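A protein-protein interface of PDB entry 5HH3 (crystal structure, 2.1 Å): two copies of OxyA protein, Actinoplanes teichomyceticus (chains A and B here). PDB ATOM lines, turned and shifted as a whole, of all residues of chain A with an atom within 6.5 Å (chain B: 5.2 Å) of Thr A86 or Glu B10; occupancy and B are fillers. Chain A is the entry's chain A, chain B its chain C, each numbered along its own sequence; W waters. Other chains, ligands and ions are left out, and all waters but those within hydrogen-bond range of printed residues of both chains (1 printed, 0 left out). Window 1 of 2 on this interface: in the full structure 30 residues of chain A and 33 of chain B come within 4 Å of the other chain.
The side-chain hydroxyl (OG1) of Thr A86 sits close to the indole nitrogen (NE1) of Trp A87, at 3.4 Å.
Ile A85 touches Ala B83. O of Thr A86 touches CG of Glu B10, 3.4 Å away. CG2 of Thr A86 touches CG1 of Val B13, at 3.7 Å. Thr A86 touches Ala B83 (O to CB, 3.5 Å). CZ3 of Trp A87 touches CB of Met B7 (3.7 Å). Trp A87 touches Glu B10. Trp A87 touches Val B14 (NE1 to CG2, 3.6 Å). Pro A88 touches Ala B82 (CG to O, 3.9 Å). Ala B83 touches Pro A88 (N to CG, 3.97 Å). Phe A90 touches Met B7.
Arg A75 touches none of the printed residues of chain B. Thr A81 touches none of the printed residues of chain B. Thr A86 touches three residues of chain B. Glu B10 touches two residues of chain A. Of the printed residues of chain A, Ile B11 touches Leu A76 and Trp A87. Of the printed residues of chain A, Val B14 touches Trp A87 (3.6 Å). The nearest residue of chain B that does not touch Thr A86 is Val B14 (4.6 Å). The nearest residue of chain A that does not touch Glu B10 is Leu A76 (6.1 Å).
Of the 11 printed residues of chain A, 6 touch a printed residue of chain B. Printed residues of chain B that touch a printed residue of chain A: Met B7, Glu B10, Ile B11, Val B13, Val B14, Ala B82 and Ala B83. Hydrophobic or aromatic side chains of chain B within 4 Å of the printed part of chain A: Met B7, Ile B11, Val B13, Val B14 and Ala B83. Among the printed residues, 12 pairs touch across the chains. Among the printed residues, no Asp or Glu carboxylate lies within 4 Å of a Lys or Arg side-chain nitrogen of the other chain.
Positions printed for both chains: 81, 82 and 83.
Water W1 lies within hydrogen-bond range of the side-chain carboxylate of Glu B10 (2.9 Å), the backbone carbonyl oxygen of Thr A86 (2.9 Å) and the backbone NH of Ala B83 (3.3 Å).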
ATOM      1  N   ARG A  75     -10.698  12.634 -28.679  1.00  0.00           N
ATOM      2  CA  ARG A  75     -10.000  13.944 -28.717  1.00  0.00           C
ATOM      3  C   ARG A  75     -10.636  14.943 -29.700  1.00  0.00           C
ATOM      4  O   ARG A  75     -11.100  14.548 -30.778  1.00  0.00           O
ATOM      5  CB  ARG A  75      -8.533  13.764 -29.145  1.00  0.00           C
ATOM      6  CG  ARG A  75      -7.687  12.863 -28.251  1.00  0.00           C
ATOM      7  CD  ARG A  75      -7.171  13.630 -27.067  1.00  0.00           C
ATOM      8  NE  ARG A  75      -6.027  14.467 -27.421  1.00  0.00           N
ATOM      9  CZ  ARG A  75      -5.771  15.688 -26.948  1.00  0.00           C
ATOM     10  NH1 ARG A  75      -6.569  16.301 -26.067  1.00  0.00           N
ATOM     11  NH2 ARG A  75      -4.692  16.322 -27.380  1.00  0.00           N
ATOM     12  N   LEU A  76     -10.616  16.230 -29.350  1.00  0.00           N
ATOM     13  CA  LEU A  76     -10.962  17.293 -30.313  1.00  0.00           C
ATOM     14  C   LEU A  76      -9.915  17.341 -31.437  1.00  0.00           C
ATOM     15  O   LEU A  76     -10.274  17.274 -32.616  1.00  0.00           O
ATOM     16  CB  LEU A  76     -11.062  18.671 -29.641  1.00  0.00           C
ATOM     17  CG  LEU A  76     -12.052  18.810 -28.470  1.00  0.00           C
ATOM     18  CD1 LEU A  76     -11.472  19.757 -27.428  1.00  0.00           C
ATOM     19  CD2 LEU A  76     -13.455  19.238 -28.880  1.00  0.00           C
ATOM     20  N   THR A  81      -1.764  19.043 -29.017  1.00  0.00           N
ATOM     21  CA  THR A  81      -1.253  19.162 -27.655  1.00  0.00           C
ATOM     22  C   THR A  81      -1.864  18.104 -26.742  1.00  0.00           C
ATOM     23  O   THR A  81      -3.058  17.844 -26.817  1.00  0.00           O
ATOM     24  CB  THR A  81      -1.551  20.557 -27.066  1.00  0.00           C
ATOM     25  OG1 THR A  81      -0.942  21.564 -27.879  1.00  0.00           O
ATOM     26  CG2 THR A  81      -1.010  20.688 -25.648  1.00  0.00           C
ATOM     27  N   ALA A  82      -1.052  17.522 -25.860  1.00  0.00           N
ATOM     28  CA  ALA A  82      -1.519  16.489 -24.922  1.00  0.00           C
ATOM     29  C   ALA A  82      -2.702  16.972 -24.074  1.00  0.00           C
ATOM     30  O   ALA A  82      -2.717  18.119 -23.622  1.00  0.00           O
ATOM     31  CB  ALA A  82      -0.374  16.043 -24.013  1.00  0.00           C
ATOM     32  N   ALA A  83      -3.675  16.088 -23.857  1.00  0.00           N
ATOM     33  CA  ALA A  83      -4.884  16.404 -23.074  1.00  0.00           C
ATOM     34  C   ALA A  83      -4.580  17.040 -21.712  1.00  0.00           C
ATOM     35  O   ALA A  83      -5.292  17.962 -21.281  1.00  0.00           O
ATOM     36  CB  ALA A  83      -5.724  15.154 -22.869  1.00  0.00           C
ATOM     37  N   GLY A  84      -3.522  16.547 -21.062  1.00  0.00           N
ATOM     38  CA  GLY A  84      -3.102  16.990 -19.733  1.00  0.00           C
ATOM     39  C   GLY A  84      -2.785  18.468 -19.550  1.00  0.00           C
ATOM     40  O   GLY A  84      -2.914  18.988 -18.442  1.00  0.00           O
ATOM     41  N   ILE A  85      -2.376  19.144 -20.621  1.00  0.00           N
ATOM     42  CA  ILE A  85      -2.044  20.576 -20.555  1.00  0.00           C
ATOM     43  C   ILE A  85      -3.298  21.458 -20.449  1.00  0.00           C
ATOM     44  O   ILE A  85      -3.431  22.224 -19.488  1.00  0.00           O
ATOM     45  CB  ILE A  85      -1.155  21.013 -21.741  1.00  0.00           C
ATOM     46  CG1 ILE A  85       0.208  20.302 -21.662  1.00  0.00           C
ATOM     47  CG2 ILE A  85      -0.957  22.534 -21.744  1.00  0.00           C
ATOM     48  CD1 ILE A  85       0.954  20.210 -22.983  1.00  0.00           C
ATOM     49  N   THR A  86      -4.207  21.352 -21.417  1.00  0.00           N
ATOM     50  CA  THR A  86      -5.398  22.213 -21.434  1.00  0.00           C
ATOM     51  C   THR A  86      -6.592  21.568 -20.726  1.00  0.00           C
ATOM     52  O   THR A  86      -7.435  22.293 -20.181  1.00  0.00           O
ATOM     53  CB  THR A  86      -5.765  22.686 -22.864  1.00  0.00           C
ATOM     54  OG1 THR A  86      -5.888  21.558 -23.725  1.00  0.00           O
ATOM     55  CG2 THR A  86      -4.694  23.574 -23.427  1.00  0.00           C
ATOM     56  N   TRP A  87      -6.644  20.230 -20.672  1.00  0.00           N
ATOM     57  CA  TRP A  87      -7.759  19.525 -20.046  1.00  0.00           C
ATOM     58  C   TRP A  87      -7.350  18.557 -18.908  1.00  0.00           C
ATOM     59  O   TRP A  87      -7.815  17.413 -18.882  1.00  0.00           O
ATOM     60  CB  TRP A  87      -8.520  18.736 -21.103  1.00  0.00           C
ATOM     61  CG  TRP A  87      -8.963  19.488 -22.313  1.00  0.00           C
ATOM     62  CD1 TRP A  87      -8.235  19.715 -23.430  1.00  0.00           C
ATOM     63  CD2 TRP A  87     -10.259  20.039 -22.555  1.00  0.00           C
ATOM     64  NE1 TRP A  87      -8.989  20.402 -24.358  1.00  0.00           N
ATOM     65  CE2 TRP A  87     -10.239  20.605 -23.841  1.00  0.00           C
ATOM     66  CE3 TRP A  87     -11.435  20.112 -21.810  1.00  0.00           C
ATOM     67  CZ2 TRP A  87     -11.348  21.254 -24.391  1.00  0.00           C
ATOM     68  CZ3 TRP A  87     -12.543  20.741 -22.371  1.00  0.00           C
ATOM     69  CH2 TRP A  87     -12.482  21.312 -23.633  1.00  0.00           C
ATOM     70  N   PRO A  88      -6.496  19.009 -17.959  1.00  0.00           N
ATOM     71  CA  PRO A  88      -6.046  18.064 -16.919  1.00  0.00           C
ATOM     72  C   PRO A  88      -7.206  17.468 -16.151  1.00  0.00           C
ATOM     73  O   PRO A  88      -8.037  18.215 -15.641  1.00  0.00           O
ATOM     74  CB  PRO A  88      -5.181  18.933 -15.987  1.00  0.00           C
ATOM     75  CG  PRO A  88      -5.487  20.351 -16.329  1.00  0.00           C
ATOM     76  CD  PRO A  88      -5.931  20.359 -17.760  1.00  0.00           C
ATOM     77  N   PHE A  90      -9.782  15.833 -17.250  1.00  0.00           N
ATOM     78  CA  PHE A  90     -11.011  15.773 -18.035  1.00  0.00           C
ATOM     79  C   PHE A  90     -10.887  14.526 -18.905  1.00  0.00           C
ATOM     80  O   PHE A  90     -10.378  14.592 -20.029  1.00  0.00           O
ATOM     81  CB  PHE A  90     -11.128  17.045 -18.900  1.00  0.00           C
ATOM     82  CG  PHE A  90     -12.528  17.357 -19.354  1.00  0.00           C
ATOM     83  CD1 PHE A  90     -13.106  16.660 -20.404  1.00  0.00           C
ATOM     84  CD2 PHE A  90     -13.272  18.359 -18.729  1.00  0.00           C
ATOM     85  CE1 PHE A  90     -14.391  16.960 -20.836  1.00  0.00           C
ATOM     86  CE2 PHE A  90     -14.563  18.652 -19.146  1.00  0.00           C
ATOM     87  CZ  PHE A  90     -15.120  17.945 -20.204  1.00  0.00           C
ATOM     88  N   MET B   7     -17.026  24.005 -21.782  1.00  0.00           N
ATOM     89  CA  MET B   7     -15.846  24.437 -21.040  1.00  0.00           C
ATOM     90  C   MET B   7     -15.245  25.646 -21.743  1.00  0.00           C
ATOM     91  O   MET B   7     -14.394  25.531 -22.618  1.00  0.00           O
ATOM     92  CB  MET B   7     -14.840  23.285 -20.930  1.00  0.00           C
ATOM     93  CG  MET B   7     -15.403  22.064 -20.231  1.00  0.00           C
ATOM     94  SD  MET B   7     -15.619  22.254 -18.448  1.00  0.00           S
ATOM     95  CE  MET B   7     -13.892  22.310 -17.976  1.00  0.00           C
ATOM     96  N   PHE B   8     -15.709  26.823 -21.330  1.00  0.00           N
ATOM     97  CA  PHE B   8     -15.499  28.074 -22.062  1.00  0.00           C
ATOM     98  C   PHE B   8     -14.057  28.451 -22.374  1.00  0.00           C
ATOM     99  O   PHE B   8     -13.696  28.704 -23.546  1.00  0.00           O
ATOM    100  CB  PHE B   8     -16.187  29.219 -21.309  1.00  0.00           C
ATOM    101  CG  PHE B   8     -16.019  30.549 -21.963  1.00  0.00           C
ATOM    102  CD1 PHE B   8     -16.590  30.807 -23.200  1.00  0.00           C
ATOM    103  CD2 PHE B   8     -15.284  31.533 -21.349  1.00  0.00           C
ATOM    104  CE1 PHE B   8     -16.406  32.049 -23.826  1.00  0.00           C
ATOM    105  CE2 PHE B   8     -15.105  32.766 -21.949  1.00  0.00           C
ATOM    106  CZ  PHE B   8     -15.660  33.026 -23.196  1.00  0.00           C
ATOM    107  N   GLU B   9     -13.229  28.522 -21.341  1.00  0.00           N
ATOM    108  CA  GLU B   9     -11.817  28.866 -21.516  1.00  0.00           C
ATOM    109  C   GLU B   9     -11.105  27.777 -22.323  1.00  0.00           C
ATOM    110  O   GLU B   9     -10.359  28.086 -23.261  1.00  0.00           O
ATOM    111  CB  GLU B   9     -11.088  29.044 -20.156  1.00  0.00           C
ATOM    112  CG  GLU B   9     -11.522  30.259 -19.336  1.00  0.00           C
ATOM    113  CD  GLU B   9     -12.813  30.078 -18.548  1.00  0.00           C
ATOM    114  OE1 GLU B   9     -13.434  28.992 -18.633  1.00  0.00           O
ATOM    115  OE2 GLU B   9     -13.219  31.026 -17.838  1.00  0.00           O
ATOM    116  N   GLU B  10     -11.354  26.512 -21.973  1.00  0.00           N
ATOM    117  CA  GLU B  10     -10.616  25.409 -22.584  1.00  0.00           C
ATOM    118  C   GLU B  10     -10.950  25.239 -24.085  1.00  0.00           C
ATOM    119  O   GLU B  10     -10.049  25.100 -24.900  1.00  0.00           O
ATOM    120  CB  GLU B  10     -10.877  24.082 -21.846  1.00  0.00           C
ATOM    121  CG  GLU B  10     -10.343  24.051 -20.418  1.00  0.00           C
ATOM    122  CD  GLU B  10     -11.313  24.625 -19.386  1.00  0.00           C
ATOM    123  OE1 GLU B  10     -12.225  25.416 -19.716  1.00  0.00           O
ATOM    124  OE2 GLU B  10     -11.184  24.255 -18.213  1.00  0.00           O
ATOM    125  N   ILE B  11     -12.236  25.217 -24.434  1.00  0.00           N
ATOM    126  CA  ILE B  11     -12.638  24.993 -25.829  1.00  0.00           C
ATOM    127  C   ILE B  11     -12.116  26.111 -26.735  1.00  0.00           C
ATOM    128  O   ILE B  11     -11.647  25.850 -27.843  1.00  0.00           O
ATOM    129  CB  ILE B  11     -14.162  24.736 -25.964  1.00  0.00           C
ATOM    130  CG1 ILE B  11     -14.483  24.071 -27.301  1.00  0.00           C
ATOM    131  CG2 ILE B  11     -14.984  26.022 -25.820  1.00  0.00           C
ATOM    132  CD1 ILE B  11     -13.922  22.680 -27.458  1.00  0.00           C
ATOM    133  N   ASN B  12     -12.099  27.344 -26.232  1.00  0.00           N
ATOM    134  CA  ASN B  12     -11.620  28.466 -27.024  1.00  0.00           C
ATOM    135  C   ASN B  12     -10.107  28.599 -27.106  1.00  0.00           C
ATOM    136  O   ASN B  12      -9.590  29.121 -28.088  1.00  0.00           O
ATOM    137  CB  ASN B  12     -12.344  29.755 -26.601  1.00  0.00           C
ATOM    138  CG  ASN B  12     -13.804  29.708 -26.994  1.00  0.00           C
ATOM    139  OD1 ASN B  12     -14.132  29.617 -28.204  1.00  0.00           O
ATOM    140  ND2 ASN B  12     -14.684  29.655 -26.008  1.00  0.00           N
ATOM    141  N   VAL B  13      -9.399  28.093 -26.106  1.00  0.00           N
ATOM    142  CA  VAL B  13      -7.944  27.861 -26.222  1.00  0.00           C
ATOM    143  C   VAL B  13      -7.636  26.879 -27.369  1.00  0.00           C
ATOM    144  O   VAL B  13      -6.752  27.127 -28.167  1.00  0.00           O
ATOM    145  CB  VAL B  13      -7.358  27.323 -24.875  1.00  0.00           C
ATOM    146  CG1 VAL B  13      -6.044  26.556 -25.058  1.00  0.00           C
ATOM    147  CG2 VAL B  13      -7.170  28.489 -23.910  1.00  0.00           C
ATOM    148  N   VAL B  14      -8.393  25.796 -27.443  1.00  0.00           N
ATOM    149  CA  VAL B  14      -8.239  24.790 -28.497  1.00  0.00           C
ATOM    150  C   VAL B  14      -8.496  25.393 -29.876  1.00  0.00           C
ATOM    151  O   VAL B  14      -7.718  25.194 -30.776  1.00  0.00           O
ATOM    152  CB  VAL B  14      -9.201  23.582 -28.295  1.00  0.00           C
ATOM    153  CG1 VAL B  14      -9.193  22.673 -29.520  1.00  0.00           C
ATOM    154  CG2 VAL B  14      -8.807  22.777 -27.071  1.00  0.00           C
ATOM    155  N   THR B  81      -9.943  28.307 -14.663  1.00  0.00           N
ATOM    156  CA  THR B  81      -9.604  27.097 -15.420  1.00  0.00           C
ATOM    157  C   THR B  81      -8.725  26.156 -14.584  1.00  0.00           C
ATOM    158  O   THR B  81      -7.835  26.612 -13.852  1.00  0.00           O
ATOM    159  CB  THR B  81      -8.794  27.448 -16.695  1.00  0.00           C
ATOM    160  OG1 THR B  81      -9.278  28.666 -17.268  1.00  0.00           O
ATOM    161  CG2 THR B  81      -8.912  26.353 -17.737  1.00  0.00           C
ATOM    162  N   ALA B  82      -8.969  24.848 -14.703  1.00  0.00           N
ATOM    163  CA  ALA B  82      -8.077  23.842 -14.116  1.00  0.00           C
ATOM    164  C   ALA B  82      -6.689  23.837 -14.790  1.00  0.00           C
ATOM    165  O   ALA B  82      -5.679  23.575 -14.137  1.00  0.00           O
ATOM    166  CB  ALA B  82      -8.712  22.457 -14.170  1.00  0.00           C
ATOM    167  N   ALA B  83      -6.646  24.138 -16.091  1.00  0.00           N
ATOM    168  CA  ALA B  83      -5.378  24.347 -16.825  1.00  0.00           C
ATOM    169  C   ALA B  83      -4.434  25.399 -16.208  1.00  0.00           C
ATOM    170  O   ALA B  83      -3.218  25.292 -16.380  1.00  0.00           O
ATOM    171  CB  ALA B  83      -5.648  24.697 -18.291  1.00  0.00           C
HETATM  172  O   HOH W   1      -8.973  22.477 -17.710  1.00  0.00           O
